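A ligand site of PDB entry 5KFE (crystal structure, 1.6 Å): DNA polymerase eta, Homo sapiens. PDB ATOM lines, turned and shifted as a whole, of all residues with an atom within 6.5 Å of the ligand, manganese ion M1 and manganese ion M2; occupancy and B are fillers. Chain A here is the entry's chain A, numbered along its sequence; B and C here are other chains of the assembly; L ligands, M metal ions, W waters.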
ATOM      1  N   ASP A  16      21.295   4.534 -27.011  1.00  0.00           N
ATOM      2  CA  ASP A  16      21.884   4.327 -25.704  1.00  0.00           C
ATOM      3  C   ASP A  16      21.060   3.384 -24.829  1.00  0.00           C
ATOM      4  O   ASP A  16      19.944   3.605 -24.658  1.00  0.00           O
ATOM      5  CB  ASP A  16      21.981   5.637 -24.972  1.00  0.00           C
ATOM      6  CG  ASP A  16      22.680   5.532 -23.692  1.00  0.00           C
ATOM      7  OD1 ASP A  16      22.055   5.371 -22.740  1.00  0.00           O
ATOM      8  OD2 ASP A  16      23.844   5.708 -23.711  1.00  0.00           O
ATOM      9  N   MET A  17      21.683   2.361 -24.309  1.00  0.00           N
ATOM     10  CA  MET A  17      20.903   1.373 -23.549  1.00  0.00           C
ATOM     11  C   MET A  17      20.340   1.945 -22.246  1.00  0.00           C
ATOM     12  O   MET A  17      20.983   2.763 -21.609  1.00  0.00           O
ATOM     13  CB  MET A  17      21.778   0.145 -23.232  1.00  0.00           C
ATOM     14  CG  MET A  17      22.424  -0.471 -24.451  1.00  0.00           C
ATOM     15  SD  MET A  17      21.280  -0.870 -25.792  1.00  0.00           S
ATOM     16  CE  MET A  17      20.287  -2.108 -25.027  1.00  0.00           C
ATOM     17  N   ASP A  18      19.142   1.564 -21.846  1.00  0.00           N
ATOM     18  CA  ASP A  18      18.586   2.030 -20.584  1.00  0.00           C
ATOM     19  C   ASP A  18      19.246   1.259 -19.436  1.00  0.00           C
ATOM     20  O   ASP A  18      19.372   0.085 -19.510  1.00  0.00           O
ATOM     21  CB  ASP A  18      17.091   1.811 -20.559  1.00  0.00           C
ATOM     22  CG  ASP A  18      16.340   2.637 -21.611  1.00  0.00           C
ATOM     23  OD1 ASP A  18      16.853   3.632 -22.072  1.00  0.00           O
ATOM     24  OD2 ASP A  18      15.266   2.271 -21.897  1.00  0.00           O
ATOM     25  N   CYS A  19      19.643   1.989 -18.402  1.00  0.00           N
ATOM     26  CA  CYS A  19      20.282   1.450 -17.184  1.00  0.00           C
ATOM     27  C   CYS A  19      20.995   0.123 -17.495  1.00  0.00           C
ATOM     28  O   CYS A  19      20.636  -0.937 -16.973  1.00  0.00           O
ATOM     29  CB  CYS A  19      19.274   1.282 -16.034  1.00  0.00           C
ATOM     30  SG  CYS A  19      17.733   0.401 -16.338  1.00  0.00           S
ATOM     31  N   PHE A  20      22.005   0.191 -18.364  1.00  0.00           N
ATOM     32  CA  PHE A  20      22.502  -0.985 -19.072  1.00  0.00           C
ATOM     33  C   PHE A  20      22.923  -2.158 -18.184  1.00  0.00           C
ATOM     34  O   PHE A  20      22.415  -3.263 -18.362  1.00  0.00           O
ATOM     35  CB  PHE A  20      23.669  -0.604 -19.998  1.00  0.00           C
ATOM     36  CG  PHE A  20      24.147  -1.745 -20.863  1.00  0.00           C
ATOM     37  CD1 PHE A  20      23.239  -2.559 -21.517  1.00  0.00           C
ATOM     38  CD2 PHE A  20      25.509  -1.979 -21.022  1.00  0.00           C
ATOM     39  CE1 PHE A  20      23.698  -3.612 -22.338  1.00  0.00           C
ATOM     40  CE2 PHE A  20      25.956  -3.020 -21.844  1.00  0.00           C
ATOM     41  CZ  PHE A  20      25.056  -3.834 -22.493  1.00  0.00           C
ATOM     42  N   PHE A  21      23.844  -1.940 -17.248  1.00  0.00           N
ATOM     43  CA  PHE A  21      24.336  -3.077 -16.453  1.00  0.00           C
ATOM     44  C   PHE A  21      23.188  -3.702 -15.654  1.00  0.00           C
ATOM     45  O   PHE A  21      23.177  -4.906 -15.412  1.00  0.00           O
ATOM     46  CB  PHE A  21      25.479  -2.681 -15.506  1.00  0.00           C
ATOM     47  CG  PHE A  21      26.785  -2.366 -16.176  1.00  0.00           C
ATOM     48  CD1 PHE A  21      26.898  -2.161 -17.554  1.00  0.00           C
ATOM     49  CD2 PHE A  21      27.927  -2.252 -15.399  1.00  0.00           C
ATOM     50  CE1 PHE A  21      28.141  -1.851 -18.131  1.00  0.00           C
ATOM     51  CE2 PHE A  21      29.168  -1.961 -15.968  1.00  0.00           C
ATOM     52  CZ  PHE A  21      29.272  -1.747 -17.330  1.00  0.00           C
ATOM     53  N   VAL A  22      22.237  -2.869 -15.199  1.00  0.00           N
ATOM     54  CA  VAL A  22      21.070  -3.393 -14.503  1.00  0.00           C
ATOM     55  C   VAL A  22      20.249  -4.294 -15.429  1.00  0.00           C
ATOM     56  O   VAL A  22      19.840  -5.393 -15.017  1.00  0.00           O
ATOM     57  CB  VAL A  22      20.197  -2.248 -13.960  1.00  0.00           C
ATOM     58  CG1 VAL A  22      18.795  -2.744 -13.570  1.00  0.00           C
ATOM     59  CG2 VAL A  22      20.888  -1.564 -12.768  1.00  0.00           C
ATOM     60  N   GLN A  41      29.902  -2.562  -7.256  1.00  0.00           N
ATOM     61  CA  GLN A  41      31.190  -3.233  -7.306  1.00  0.00           C
ATOM     62  C   GLN A  41      31.836  -3.167  -5.931  1.00  0.00           C
ATOM     63  O   GLN A  41      31.793  -2.136  -5.261  1.00  0.00           O
ATOM     64  CB  GLN A  41      32.108  -2.668  -8.387  1.00  0.00           C
ATOM     65  CG  GLN A  41      32.278  -1.180  -8.392  1.00  0.00           C
ATOM     66  CD  GLN A  41      32.964  -0.703  -9.664  1.00  0.00           C
ATOM     67  OE1 GLN A  41      33.124  -1.460 -10.624  1.00  0.00           O
ATOM     68  NE2 GLN A  41      33.379   0.547  -9.668  1.00  0.00           N
ATOM     69  N   ILE A  51      27.188   1.500  -9.616  1.00  0.00           N
ATOM     70  CA  ILE A  51      27.572   1.981 -10.941  1.00  0.00           C
ATOM     71  C   ILE A  51      26.408   1.983 -11.944  1.00  0.00           C
ATOM     72  O   ILE A  51      26.542   2.530 -13.030  1.00  0.00           O
ATOM     73  CB  ILE A  51      28.740   1.159 -11.543  1.00  0.00           C
ATOM     74  CG1 ILE A  51      28.394  -0.328 -11.654  1.00  0.00           C
ATOM     75  CG2 ILE A  51      30.008   1.381 -10.697  1.00  0.00           C
ATOM     76  CD1 ILE A  51      29.476  -1.129 -12.393  1.00  0.00           C
ATOM     77  N   ALA A  52      25.257   1.412 -11.583  1.00  0.00           N
ATOM     78  CA  ALA A  52      24.075   1.461 -12.456  1.00  0.00           C
ATOM     79  C   ALA A  52      22.813   1.311 -11.616  1.00  0.00           C
ATOM     80  O   ALA A  52      22.826   0.596 -10.610  1.00  0.00           O
ATOM     81  CB  ALA A  52      24.138   0.366 -13.550  1.00  0.00           C
ATOM     82  N   VAL A  53      21.737   1.986 -12.016  1.00  0.00           N
ATOM     83  CA  VAL A  53      20.534   2.104 -11.194  1.00  0.00           C
ATOM     84  C   VAL A  53      19.272   1.969 -12.043  1.00  0.00           C
ATOM     85  O   VAL A  53      19.133   2.701 -13.030  1.00  0.00           O
ATOM     86  CB  VAL A  53      20.482   3.480 -10.469  1.00  0.00           C
ATOM     87  CG1 VAL A  53      19.338   3.530  -9.475  1.00  0.00           C
ATOM     88  CG2 VAL A  53      21.791   3.785  -9.771  1.00  0.00           C
ATOM     89  N   TYR A  55      15.306   2.395 -13.119  1.00  0.00           N
ATOM     90  CA  TYR A  55      14.477   3.598 -13.040  1.00  0.00           C
ATOM     91  C   TYR A  55      13.558   3.566 -11.820  1.00  0.00           C
ATOM     92  O   TYR A  55      13.275   4.610 -11.235  1.00  0.00           O
ATOM     93  CB  TYR A  55      13.705   3.791 -14.345  1.00  0.00           C
ATOM     94  CG  TYR A  55      14.617   4.391 -15.397  1.00  0.00           C
ATOM     95  CD1 TYR A  55      15.503   3.598 -16.115  1.00  0.00           C
ATOM     96  CD2 TYR A  55      14.642   5.762 -15.604  1.00  0.00           C
ATOM     97  CE1 TYR A  55      16.370   4.141 -17.036  1.00  0.00           C
ATOM     98  CE2 TYR A  55      15.507   6.326 -16.524  1.00  0.00           C
ATOM     99  CZ  TYR A  55      16.369   5.518 -17.236  1.00  0.00           C
ATOM    100  OH  TYR A  55      17.217   6.100 -18.150  1.00  0.00           O
ATOM    101  N   ARG A  58      15.774   4.879  -9.119  1.00  0.00           N
ATOM    102  CA  ARG A  58      16.025   6.315  -9.266  1.00  0.00           C
ATOM    103  C   ARG A  58      14.913   7.159  -8.643  1.00  0.00           C
ATOM    104  O   ARG A  58      15.176   8.267  -8.165  1.00  0.00           O
ATOM    105  CB  ARG A  58      16.191   6.691 -10.740  1.00  0.00           C
ATOM    106  CG  ARG A  58      17.343   6.003 -11.395  1.00  0.00           C
ATOM    107  CD  ARG A  58      17.523   6.451 -12.822  1.00  0.00           C
ATOM    108  NE  ARG A  58      18.419   5.511 -13.496  1.00  0.00           N
ATOM    109  CZ  ARG A  58      18.969   5.712 -14.691  1.00  0.00           C
ATOM    110  NH1 ARG A  58      18.746   6.841 -15.350  1.00  0.00           N
ATOM    111  NH2 ARG A  58      19.779   4.765 -15.208  1.00  0.00           N
ATOM    112  N   ARG A  64      24.184   6.711  -9.352  1.00  0.00           N
ATOM    113  CA  ARG A  64      25.548   6.261  -9.549  1.00  0.00           C
ATOM    114  C   ARG A  64      26.478   6.991  -8.571  1.00  0.00           C
ATOM    115  O   ARG A  64      26.196   8.126  -8.186  1.00  0.00           O
ATOM    116  CB  ARG A  64      25.949   6.502 -11.018  1.00  0.00           C
ATOM    117  CG  ARG A  64      27.426   6.397 -11.342  1.00  0.00           C
ATOM    118  CD  ARG A  64      27.608   6.523 -12.855  1.00  0.00           C
ATOM    119  NE  ARG A  64      26.873   5.444 -13.497  1.00  0.00           N
ATOM    120  CZ  ARG A  64      26.031   5.582 -14.522  1.00  0.00           C
ATOM    121  NH1 ARG A  64      25.794   6.768 -15.079  1.00  0.00           N
ATOM    122  NH2 ARG A  64      25.411   4.510 -14.999  1.00  0.00           N
ATOM    123  N   LEU A  92      34.602  -6.782 -15.838  1.00  0.00           N
ATOM    124  CA  LEU A  92      33.418  -6.303 -16.555  1.00  0.00           C
ATOM    125  C   LEU A  92      33.050  -7.116 -17.796  1.00  0.00           C
ATOM    126  O   LEU A  92      32.280  -6.659 -18.641  1.00  0.00           O
ATOM    127  CB  LEU A  92      33.616  -4.830 -16.944  1.00  0.00           C
ATOM    128  CG  LEU A  92      34.020  -3.924 -15.781  1.00  0.00           C
ATOM    129  CD1 LEU A  92      34.326  -2.532 -16.292  1.00  0.00           C
ATOM    130  CD2 LEU A  92      32.901  -3.903 -14.744  1.00  0.00           C
ATOM    131  N   SER A 116      30.592   4.186 -26.345  1.00  0.00           N
ATOM    132  CA  SER A 116      30.789   3.717 -24.977  1.00  0.00           C
ATOM    133  C   SER A 116      30.396   2.244 -24.920  1.00  0.00           C
ATOM    134  O   SER A 116      29.981   1.673 -25.921  1.00  0.00           O
ATOM    135  CB  SER A 116      29.952   4.504 -23.973  1.00  0.00           C
ATOM    136  OG  SER A 116      28.608   4.032 -23.942  1.00  0.00           O
ATOM    137  N   ILE A 117      30.474   1.649 -23.735  1.00  0.00           N
ATOM    138  CA  ILE A 117      30.060   0.264 -23.609  1.00  0.00           C
ATOM    139  C   ILE A 117      28.560   0.091 -23.916  1.00  0.00           C
ATOM    140  O   ILE A 117      28.111  -1.000 -24.245  1.00  0.00           O
ATOM    141  CB  ILE A 117      30.398  -0.267 -22.178  1.00  0.00           C
ATOM    142  CG1 ILE A 117      30.387  -1.788 -22.164  1.00  0.00           C
ATOM    143  CG2 ILE A 117      29.443   0.331 -21.143  1.00  0.00           C
ATOM    144  CD1 ILE A 117      31.034  -2.372 -20.893  1.00  0.00           C
ATOM    145  N   ASP A 118      27.768   1.161 -23.822  1.00  0.00           N
ATOM    146  CA  ASP A 118      26.331   0.984 -24.013  1.00  0.00           C
ATOM    147  C   ASP A 118      25.695   1.913 -25.039  1.00  0.00           C
ATOM    148  O   ASP A 118      24.473   2.069 -25.062  1.00  0.00           O
ATOM    149  CB  ASP A 118      25.583   1.130 -22.671  1.00  0.00           C
ATOM    150  CG  ASP A 118      25.148   2.568 -22.382  1.00  0.00           C
ATOM    151  OD1 ASP A 118      25.900   3.548 -22.632  1.00  0.00           O
ATOM    152  OD2 ASP A 118      23.969   2.707 -21.939  1.00  0.00           O
ATOM    153  N   GLU A 119      26.504   2.532 -25.906  1.00  0.00           N
ATOM    154  CA  GLU A 119      25.923   3.402 -26.920  1.00  0.00           C
ATOM    155  C   GLU A 119      26.742   3.512 -28.176  1.00  0.00           C
ATOM    156  O   GLU A 119      27.970   3.329 -28.161  1.00  0.00           O
ATOM    157  CB  GLU A 119      25.683   4.804 -26.357  1.00  0.00           C
ATOM    158  CG  GLU A 119      26.934   5.654 -26.208  1.00  0.00           C
ATOM    159  CD  GLU A 119      26.770   6.648 -25.081  1.00  0.00           C
ATOM    160  OE1 GLU A 119      26.487   7.834 -25.347  1.00  0.00           O
ATOM    161  OE2 GLU A 119      26.890   6.227 -23.912  1.00  0.00           O
ATOM    162  N   SER A 216      17.046   3.819 -25.467  1.00  0.00           N
ATOM    163  CA  SER A 216      16.491   5.075 -25.955  1.00  0.00           C
ATOM    164  C   SER A 216      17.321   5.526 -27.129  1.00  0.00           C
ATOM    165  O   SER A 216      18.377   4.973 -27.377  1.00  0.00           O
ATOM    166  CB  SER A 216      16.492   6.112 -24.843  1.00  0.00           C
ATOM    167  OG  SER A 216      15.654   5.670 -23.780  1.00  0.00           O
ATOM    168  N   LYS A 227      22.848  12.940 -29.472  1.00  0.00           N
ATOM    169  CA  LYS A 227      23.104  12.582 -28.078  1.00  0.00           C
ATOM    170  C   LYS A 227      22.183  13.358 -27.130  1.00  0.00           C
ATOM    171  O   LYS A 227      21.623  12.780 -26.201  1.00  0.00           O
ATOM    172  CB  LYS A 227      24.579  12.848 -27.720  1.00  0.00           C
ATOM    173  CG  LYS A 227      24.899  12.580 -26.247  1.00  0.00           C
ATOM    174  CD  LYS A 227      24.647  11.129 -25.825  1.00  0.00           C
ATOM    175  CE  LYS A 227      25.033  10.924 -24.359  1.00  0.00           C
ATOM    176  NZ  LYS A 227      24.939   9.508 -23.875  1.00  0.00           N
ATOM    177  N   LYS A 234      14.068   9.484 -22.001  1.00  0.00           N
ATOM    178  CA  LYS A 234      14.350   8.139 -21.462  1.00  0.00           C
ATOM    179  C   LYS A 234      13.429   7.744 -20.295  1.00  0.00           C
ATOM    180  O   LYS A 234      13.014   8.599 -19.612  1.00  0.00           O
ATOM    181  CB  LYS A 234      15.830   8.051 -21.107  1.00  0.00           C
ATOM    182  CG  LYS A 234      16.288   9.168 -20.277  1.00  0.00           C
ATOM    183  CD  LYS A 234      17.781   9.071 -19.986  1.00  0.00           C
ATOM    184  CE  LYS A 234      18.058   9.289 -18.500  1.00  0.00           C
ATOM    185  NZ  LYS A 234      19.527   9.268 -18.300  1.00  0.00           N
ATOM    186  N   PRO A 235      13.185   6.465 -20.036  1.00  0.00           N
ATOM    187  CA  PRO A 235      13.718   5.328 -20.794  1.00  0.00           C
ATOM    188  C   PRO A 235      12.767   4.835 -21.870  1.00  0.00           C
ATOM    189  O   PRO A 235      11.598   5.246 -21.919  1.00  0.00           O
ATOM    190  CB  PRO A 235      13.865   4.259 -19.714  1.00  0.00           C
ATOM    191  CG  PRO A 235      12.670   4.517 -18.821  1.00  0.00           C
ATOM    192  CD  PRO A 235      12.463   6.031 -18.832  1.00  0.00           C
ATOM    193  P    DT B   8      28.696  11.203 -20.699  1.00  0.00           P
ATOM    194  OP1  DT B   8      27.409  11.419 -21.402  1.00  0.00           O
ATOM    195  OP2  DT B   8      28.843  11.604 -19.270  1.00  0.00           O
ATOM    196  O5'  DT B   8      29.122   9.652 -20.769  1.00  0.00           O
ATOM    197  C5'  DT B   8      29.034   8.811 -21.996  1.00  0.00           C
ATOM    198  C4'  DT B   8      29.225   7.366 -21.572  1.00  0.00           C
ATOM    199  O4'  DT B   8      30.441   7.382 -20.790  1.00  0.00           O
ATOM    200  C3'  DT B   8      28.089   6.951 -20.635  1.00  0.00           C
ATOM    201  O3'  DT B   8      27.547   5.688 -21.042  1.00  0.00           O
ATOM    202  C2'  DT B   8      28.752   6.875 -19.251  1.00  0.00           C
ATOM    203  C1'  DT B   8      30.228   6.681 -19.581  1.00  0.00           C
ATOM    204  N1   DT B   8      31.151   7.217 -18.543  1.00  0.00           N
ATOM    205  C2   DT B   8      32.032   6.357 -17.931  1.00  0.00           C
ATOM    206  O2   DT B   8      32.100   5.179 -18.191  1.00  0.00           O
ATOM    207  N3   DT B   8      32.837   6.943 -16.977  1.00  0.00           N
ATOM    208  C4   DT B   8      32.854   8.257 -16.599  1.00  0.00           C
ATOM    209  O4   DT B   8      33.613   8.683 -15.727  1.00  0.00           O
ATOM    210  C5   DT B   8      31.905   9.112 -17.273  1.00  0.00           C
ATOM    211  C7   DT B   8      31.832  10.577 -16.938  1.00  0.00           C
ATOM    212  C6   DT B   8      31.111   8.554 -18.211  1.00  0.00           C
ATOM    213  P    DT C   3      35.094   8.964  -1.872  1.00  0.00           P
ATOM    214  OP1  DT C   3      36.155   9.985  -1.962  1.00  0.00           O
ATOM    215  OP2  DT C   3      33.898   9.187  -1.036  1.00  0.00           O
ATOM    216  O5'  DT C   3      34.598   8.627  -3.361  1.00  0.00           O
ATOM    217  C5'  DT C   3      33.785   7.500  -3.604  1.00  0.00           C
ATOM    218  C4'  DT C   3      33.702   7.212  -5.080  1.00  0.00           C
ATOM    219  O4'  DT C   3      32.750   8.116  -5.693  1.00  0.00           O
ATOM    220  C3'  DT C   3      35.025   7.402  -5.828  1.00  0.00           C
ATOM    221  O3'  DT C   3      35.428   6.183  -6.441  1.00  0.00           O
ATOM    222  C2'  DT C   3      34.733   8.505  -6.857  1.00  0.00           C
ATOM    223  C1'  DT C   3      33.215   8.486  -6.963  1.00  0.00           C
ATOM    224  N1   DT C   3      32.624   9.798  -7.310  1.00  0.00           N
ATOM    225  C2   DT C   3      31.885   9.922  -8.457  1.00  0.00           C
ATOM    226  O2   DT C   3      31.685   8.990  -9.219  1.00  0.00           O
ATOM    227  N3   DT C   3      31.381  11.172  -8.683  1.00  0.00           N
ATOM    228  C4   DT C   3      31.543  12.293  -7.878  1.00  0.00           C
ATOM    229  O4   DT C   3      31.049  13.374  -8.161  1.00  0.00           O
ATOM    230  C5   DT C   3      32.332  12.093  -6.686  1.00  0.00           C
ATOM    231  C7   DT C   3      32.581  13.234  -5.750  1.00  0.00           C
ATOM    232  C6   DT C   3      32.834  10.865  -6.460  1.00  0.00           C
ATOM    233  P    DT C   4      36.825   5.514  -5.983  1.00  0.00           P
ATOM    234  OP1  DT C   4      36.742   5.229  -4.546  1.00  0.00           O
ATOM    235  OP2  DT C   4      37.889   6.388  -6.516  1.00  0.00           O
ATOM    236  O5'  DT C   4      36.905   4.141  -6.821  1.00  0.00           O
ATOM    237  C5'  DT C   4      36.291   2.941  -6.336  1.00  0.00           C
ATOM    238  C4'  DT C   4      36.142   1.952  -7.496  1.00  0.00           C
ATOM    239  O4'  DT C   4      35.231   2.537  -8.453  1.00  0.00           O
ATOM    240  C3'  DT C   4      37.435   1.692  -8.254  1.00  0.00           C
ATOM    241  O3'  DT C   4      37.416   0.346  -8.706  1.00  0.00           O
ATOM    242  C2'  DT C   4      37.353   2.689  -9.423  1.00  0.00           C
ATOM    243  C1'  DT C   4      35.870   2.652  -9.715  1.00  0.00           C
ATOM    244  N1   DT C   4      35.292   3.844 -10.361  1.00  0.00           N
ATOM    245  C2   DT C   4      34.296   3.629 -11.266  1.00  0.00           C
ATOM    246  O2   DT C   4      33.930   2.513 -11.596  1.00  0.00           O
ATOM    247  N3   DT C   4      33.765   4.762 -11.802  1.00  0.00           N
ATOM    248  C4   DT C   4      34.091   6.068 -11.506  1.00  0.00           C
ATOM    249  O4   DT C   4      33.532   7.015 -12.050  1.00  0.00           O
ATOM    250  C5   DT C   4      35.138   6.232 -10.519  1.00  0.00           C
ATOM    251  C7   DT C   4      35.595   7.606 -10.118  1.00  0.00           C
ATOM    252  C6   DT C   4      35.674   5.113  -9.974  1.00  0.00           C
ATOM    253  P    DA C   5      38.635  -0.260  -9.556  1.00  0.00           P
ATOM    254  OP1  DA C   5      38.827  -1.646  -9.099  1.00  0.00           O
ATOM    255  OP2  DA C   5      39.758   0.707  -9.543  1.00  0.00           O
ATOM    256  O5'  DA C   5      38.087  -0.265 -11.034  1.00  0.00           O
ATOM    257  C5'  DA C   5      37.020  -1.146 -11.390  1.00  0.00           C
ATOM    258  C4'  DA C   5      36.751  -1.053 -12.868  1.00  0.00           C
ATOM    259  O4'  DA C   5      36.170   0.245 -13.190  1.00  0.00           O
ATOM    260  C3'  DA C   5      37.988  -1.192 -13.749  1.00  0.00           C
ATOM    261  O3'  DA C   5      37.645  -1.927 -14.902  1.00  0.00           O
ATOM    262  C2'  DA C   5      38.328   0.261 -14.081  1.00  0.00           C
ATOM    263  C1'  DA C   5      36.916   0.833 -14.231  1.00  0.00           C
ATOM    264  N9   DA C   5      36.841   2.276 -14.076  1.00  0.00           N
ATOM    265  C8   DA C   5      37.582   3.064 -13.239  1.00  0.00           C
ATOM    266  N7   DA C   5      37.257   4.336 -13.295  1.00  0.00           N
ATOM    267  C5   DA C   5      36.239   4.384 -14.236  1.00  0.00           C
ATOM    268  C6   DA C   5      35.477   5.450 -14.759  1.00  0.00           C
ATOM    269  N6   DA C   5      35.642   6.721 -14.373  1.00  0.00           N
ATOM    270  N1   DA C   5      34.544   5.151 -15.684  1.00  0.00           N
ATOM    271  C2   DA C   5      34.381   3.875 -16.053  1.00  0.00           C
ATOM    272  N3   DA C   5      35.046   2.789 -15.641  1.00  0.00           N
ATOM    273  C4   DA C   5      35.965   3.123 -14.716  1.00  0.00           C
HETATM  274  P1  LIG L   1      20.683   5.475 -18.549  1.00  0.00           P
HETATM  275  O1  LIG L   1      20.522   6.811 -17.829  1.00  0.00           O
HETATM  276  O2  LIG L   1      19.359   4.826 -18.821  1.00  0.00           O
HETATM  277  O3  LIG L   1      21.498   5.629 -19.805  1.00  0.00           O
HETATM  278  P2  LIG L   1      22.864   3.801 -17.803  1.00  0.00           P
HETATM  279  O4  LIG L   1      22.809   3.002 -19.097  1.00  0.00           O
HETATM  280  O5  LIG L   1      23.183   2.942 -16.606  1.00  0.00           O
HETATM  281  O6  LIG L   1      21.452   4.520 -17.533  1.00  0.00           O
HETATM  282  P3  LIG L   1      25.079   5.247 -18.926  1.00  0.00           P
HETATM  283  O7  LIG L   1      25.675   6.577 -18.522  1.00  0.00           O
HETATM  284  O8  LIG L   1      24.580   5.237 -20.347  1.00  0.00           O
HETATM  285  O9  LIG L   1      23.920   4.978 -17.863  1.00  0.00           O
HETATM  286  O10 LIG L   1      26.177   4.144 -18.697  1.00  0.00           O
HETATM  287  C1  LIG L   1      26.089   2.847 -19.240  1.00  0.00           C
HETATM  288  C2  LIG L   1      26.727   1.811 -18.309  1.00  0.00           C
HETATM  289  O11 LIG L   1      28.089   2.136 -18.189  1.00  0.00           O
HETATM  290  C3  LIG L   1      26.157   1.832 -16.962  1.00  0.00           C
HETATM  291  O12 LIG L   1      25.058   0.920 -16.838  1.00  0.00           O
HETATM  292  C4  LIG L   1      27.263   1.431 -16.091  1.00  0.00           C
HETATM  293  C5  LIG L   1      28.472   1.945 -16.820  1.00  0.00           C
HETATM  294  N1  LIG L   1      28.945   3.176 -16.284  1.00  0.00           N
HETATM  295  C6  LIG L   1      28.502   4.431 -16.578  1.00  0.00           C
HETATM  296  N2  LIG L   1      29.180   5.340 -15.893  1.00  0.00           N
HETATM  297  C7  LIG L   1      30.099   4.716 -15.153  1.00  0.00           C
HETATM  298  C8  LIG L   1      31.085   5.127 -14.255  1.00  0.00           C
HETATM  299  N3  LIG L   1      31.240   6.510 -13.972  1.00  0.00           N
HETATM  300  N4  LIG L   1      31.851   4.213 -13.657  1.00  0.00           N
HETATM  301  C9  LIG L   1      31.722   2.890 -13.892  1.00  0.00           C
HETATM  302  N5  LIG L   1      30.776   2.446 -14.775  1.00  0.00           N
HETATM  303  C10 LIG L   1      29.976   3.335 -15.392  1.00  0.00           C
HETATM  304 MN    MN M   1      25.592   5.641 -22.306  1.00  0.00          MN
HETATM  305 MN    MN M   2      22.619   4.071 -21.015  1.00  0.00          MN
HETATM  306  O   HOH W   1      22.150   7.872 -16.042  1.00  0.00           O
HETATM  307  O   HOH W   2      29.068   3.732 -20.409  1.00  0.00           O
HETATM  308  O   HOH W   3      22.275   3.692 -14.198  1.00  0.00           O
HETATM  309  O   HOH W   4      29.051   8.204 -15.496  1.00  0.00           O
HETATM  310  O   HOH W   5      22.538   7.978 -20.654  1.00  0.00           O
HETATM  311  O   HOH W   6      31.858  -0.050 -15.415  1.00  0.00           O
HETATM  312  O   HOH W   7      31.509   2.490 -18.529  1.00  0.00           O
HETATM  313  O   HOH W   8      25.170   7.675 -21.723  1.00  0.00           O
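Water W8 lies within hydrogen-bond range of NZ of Lys 227 and O7 of the ligand.
Water W7 lies within hydrogen-bond range of O2 of DT 8 of chain B and an oxygen (O11) of the ligand.
N3 of the ligand is in hydrogen-bond range of N3 of DT 8 of chain B, at 3.4 Å.
An oxygen (O2) of the ligand lies within hydrogen-bond range of the side-chain hydroxyl (OH) of Tyr 55.
O1 of the ligand is in salt-bridge range of NZ of Lys 234 (2.7 Å).
O4 of DT 4 of chain C is in hydrogen-bond range of N3 of the ligand, at 3.0 Å.
NH1 of Arg 58 is in salt-bridge range of O1 of the ligand (3.0 Å).
The backbone NH of Cys 19 is in hydrogen-bond range of an oxygen (O2) of the ligand (2.9 Å).
O5 of the ligand is in hydrogen-bond range of N of Phe 20, at 3.5 Å.
An oxygen (O12) of the ligand sits at hydrogen-bond distance from the backbone NH (N) of Phe 21, 3.1 Å away.
The guanidinium group (NH2) of Arg 64 lies within salt-bridge range of an oxygen (O5) of the ligand, at 3.2 Å.
N1 of DA 5 of chain C sits close to a nitrogen (N4) of the ligand (3.5 Å).
Residues that only touch the ligand: Asp 18 (3.4 Å), Ile 51 (3.3 Å), Ala 52 (3.5 Å) and Ile 117 (3.7 Å).
Hydrophobic or aromatic side chains that line the ligand: Phe 20, Phe 21, Ile 51, Ala 52, Tyr 55 and Ile 117.
17 residues have an atom within 4 Å of the ligand: Asp 16, Met 17, Asp 18, Cys 19, Phe 20, Phe 21, Ile 51, Ala 52, Tyr 55, Arg 58, Arg 64, Ile 117, Asp 118, Lys 234, DT 8 of chain B, DT 4 of chain C and DA 5 of chain C.
The nearest printed residue that does not touch the ligand is Glu 119 (4.4 Å).
The backbone NH of Glu 119 sits at hydrogen-bond distance from the side-chain hydroxyl of Ser 116, at 3.2 Å.
OE1 of Glu 119 is in salt-bridge range of NZ of Lys 227, 2.7 Å away.
The side-chain carboxylate (OD2) of Asp 16 sits close to the side-chain amino group (NZ) of Lys 227.
NZ of Lys 227 lies within salt-bridge range of OP1 of DT 8 of chain B (3.98 Å).
OH of Tyr 55 is in hydrogen-bond range of NH1 of Arg 58, 3.3 Å away.
O2 of DT 4 of chain C is in hydrogen-bond range of the side-chain amide nitrogen of Gln 41 (2.8 Å).
The guanidinium group of Arg 58 lies within hydrogen-bond range of the backbone carbonyl oxygen of Val 53 (2.9 Å).
The guanidinium group (NE) of Arg 64 lies within hydrogen-bond range of the backbone carbonyl oxygen (O) of Ile 51, 3.0 Å away.
Manganese ion M2 is bound by the side-chain carboxylate (OD2) of Asp 118 (2.1 Å), the backbone carbonyl oxygen (O) of Met 17 (2.2 Å), an oxygen (O4) of the ligand (2.2 Å), the side-chain carboxylate (OD1) of Asp 16 (2.2 Å), an oxygen (O3) of the ligand (2.3 Å) and an oxygen (O8) of the ligand (2.4 Å).
Manganese ion M2 has six donor atoms within binding distance.
Manganese ion M1 is bound by OD1 of Asp 118, 2.1 Å away.
The side-chain carboxylate (OE2) of Glu 119 is bound to manganese ion M1 (2.1 Å).
Manganese ion M1 is bound by water W8 (2.2 Å).
O8 of the ligand binds manganese ion M1.
Manganese ion M1 is bound by OD2 of Asp 16.
O3' of DT 8 of chain B is bound to manganese ion M1, 2.3 Å away.
Manganese ion M1 has six donor atoms within binding distance.
Ser 116 touches manganese ion M1 (OG to MN, 3.8 Å).
Within 4 Å of manganese ion M1: Asp 16, Ser 116, Asp 118, Glu 119 and DT 8 of chain B.
Along chain A the residues within 4 Å of manganese ion M1 span positions 16 to 119.
The nearest printed residue that does not touch manganese ion M1 is Lys 227 (4.2 Å).
Three residues have an atom within 4 Å of manganese ion M2: Asp 16, Met 17 and Asp 118.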
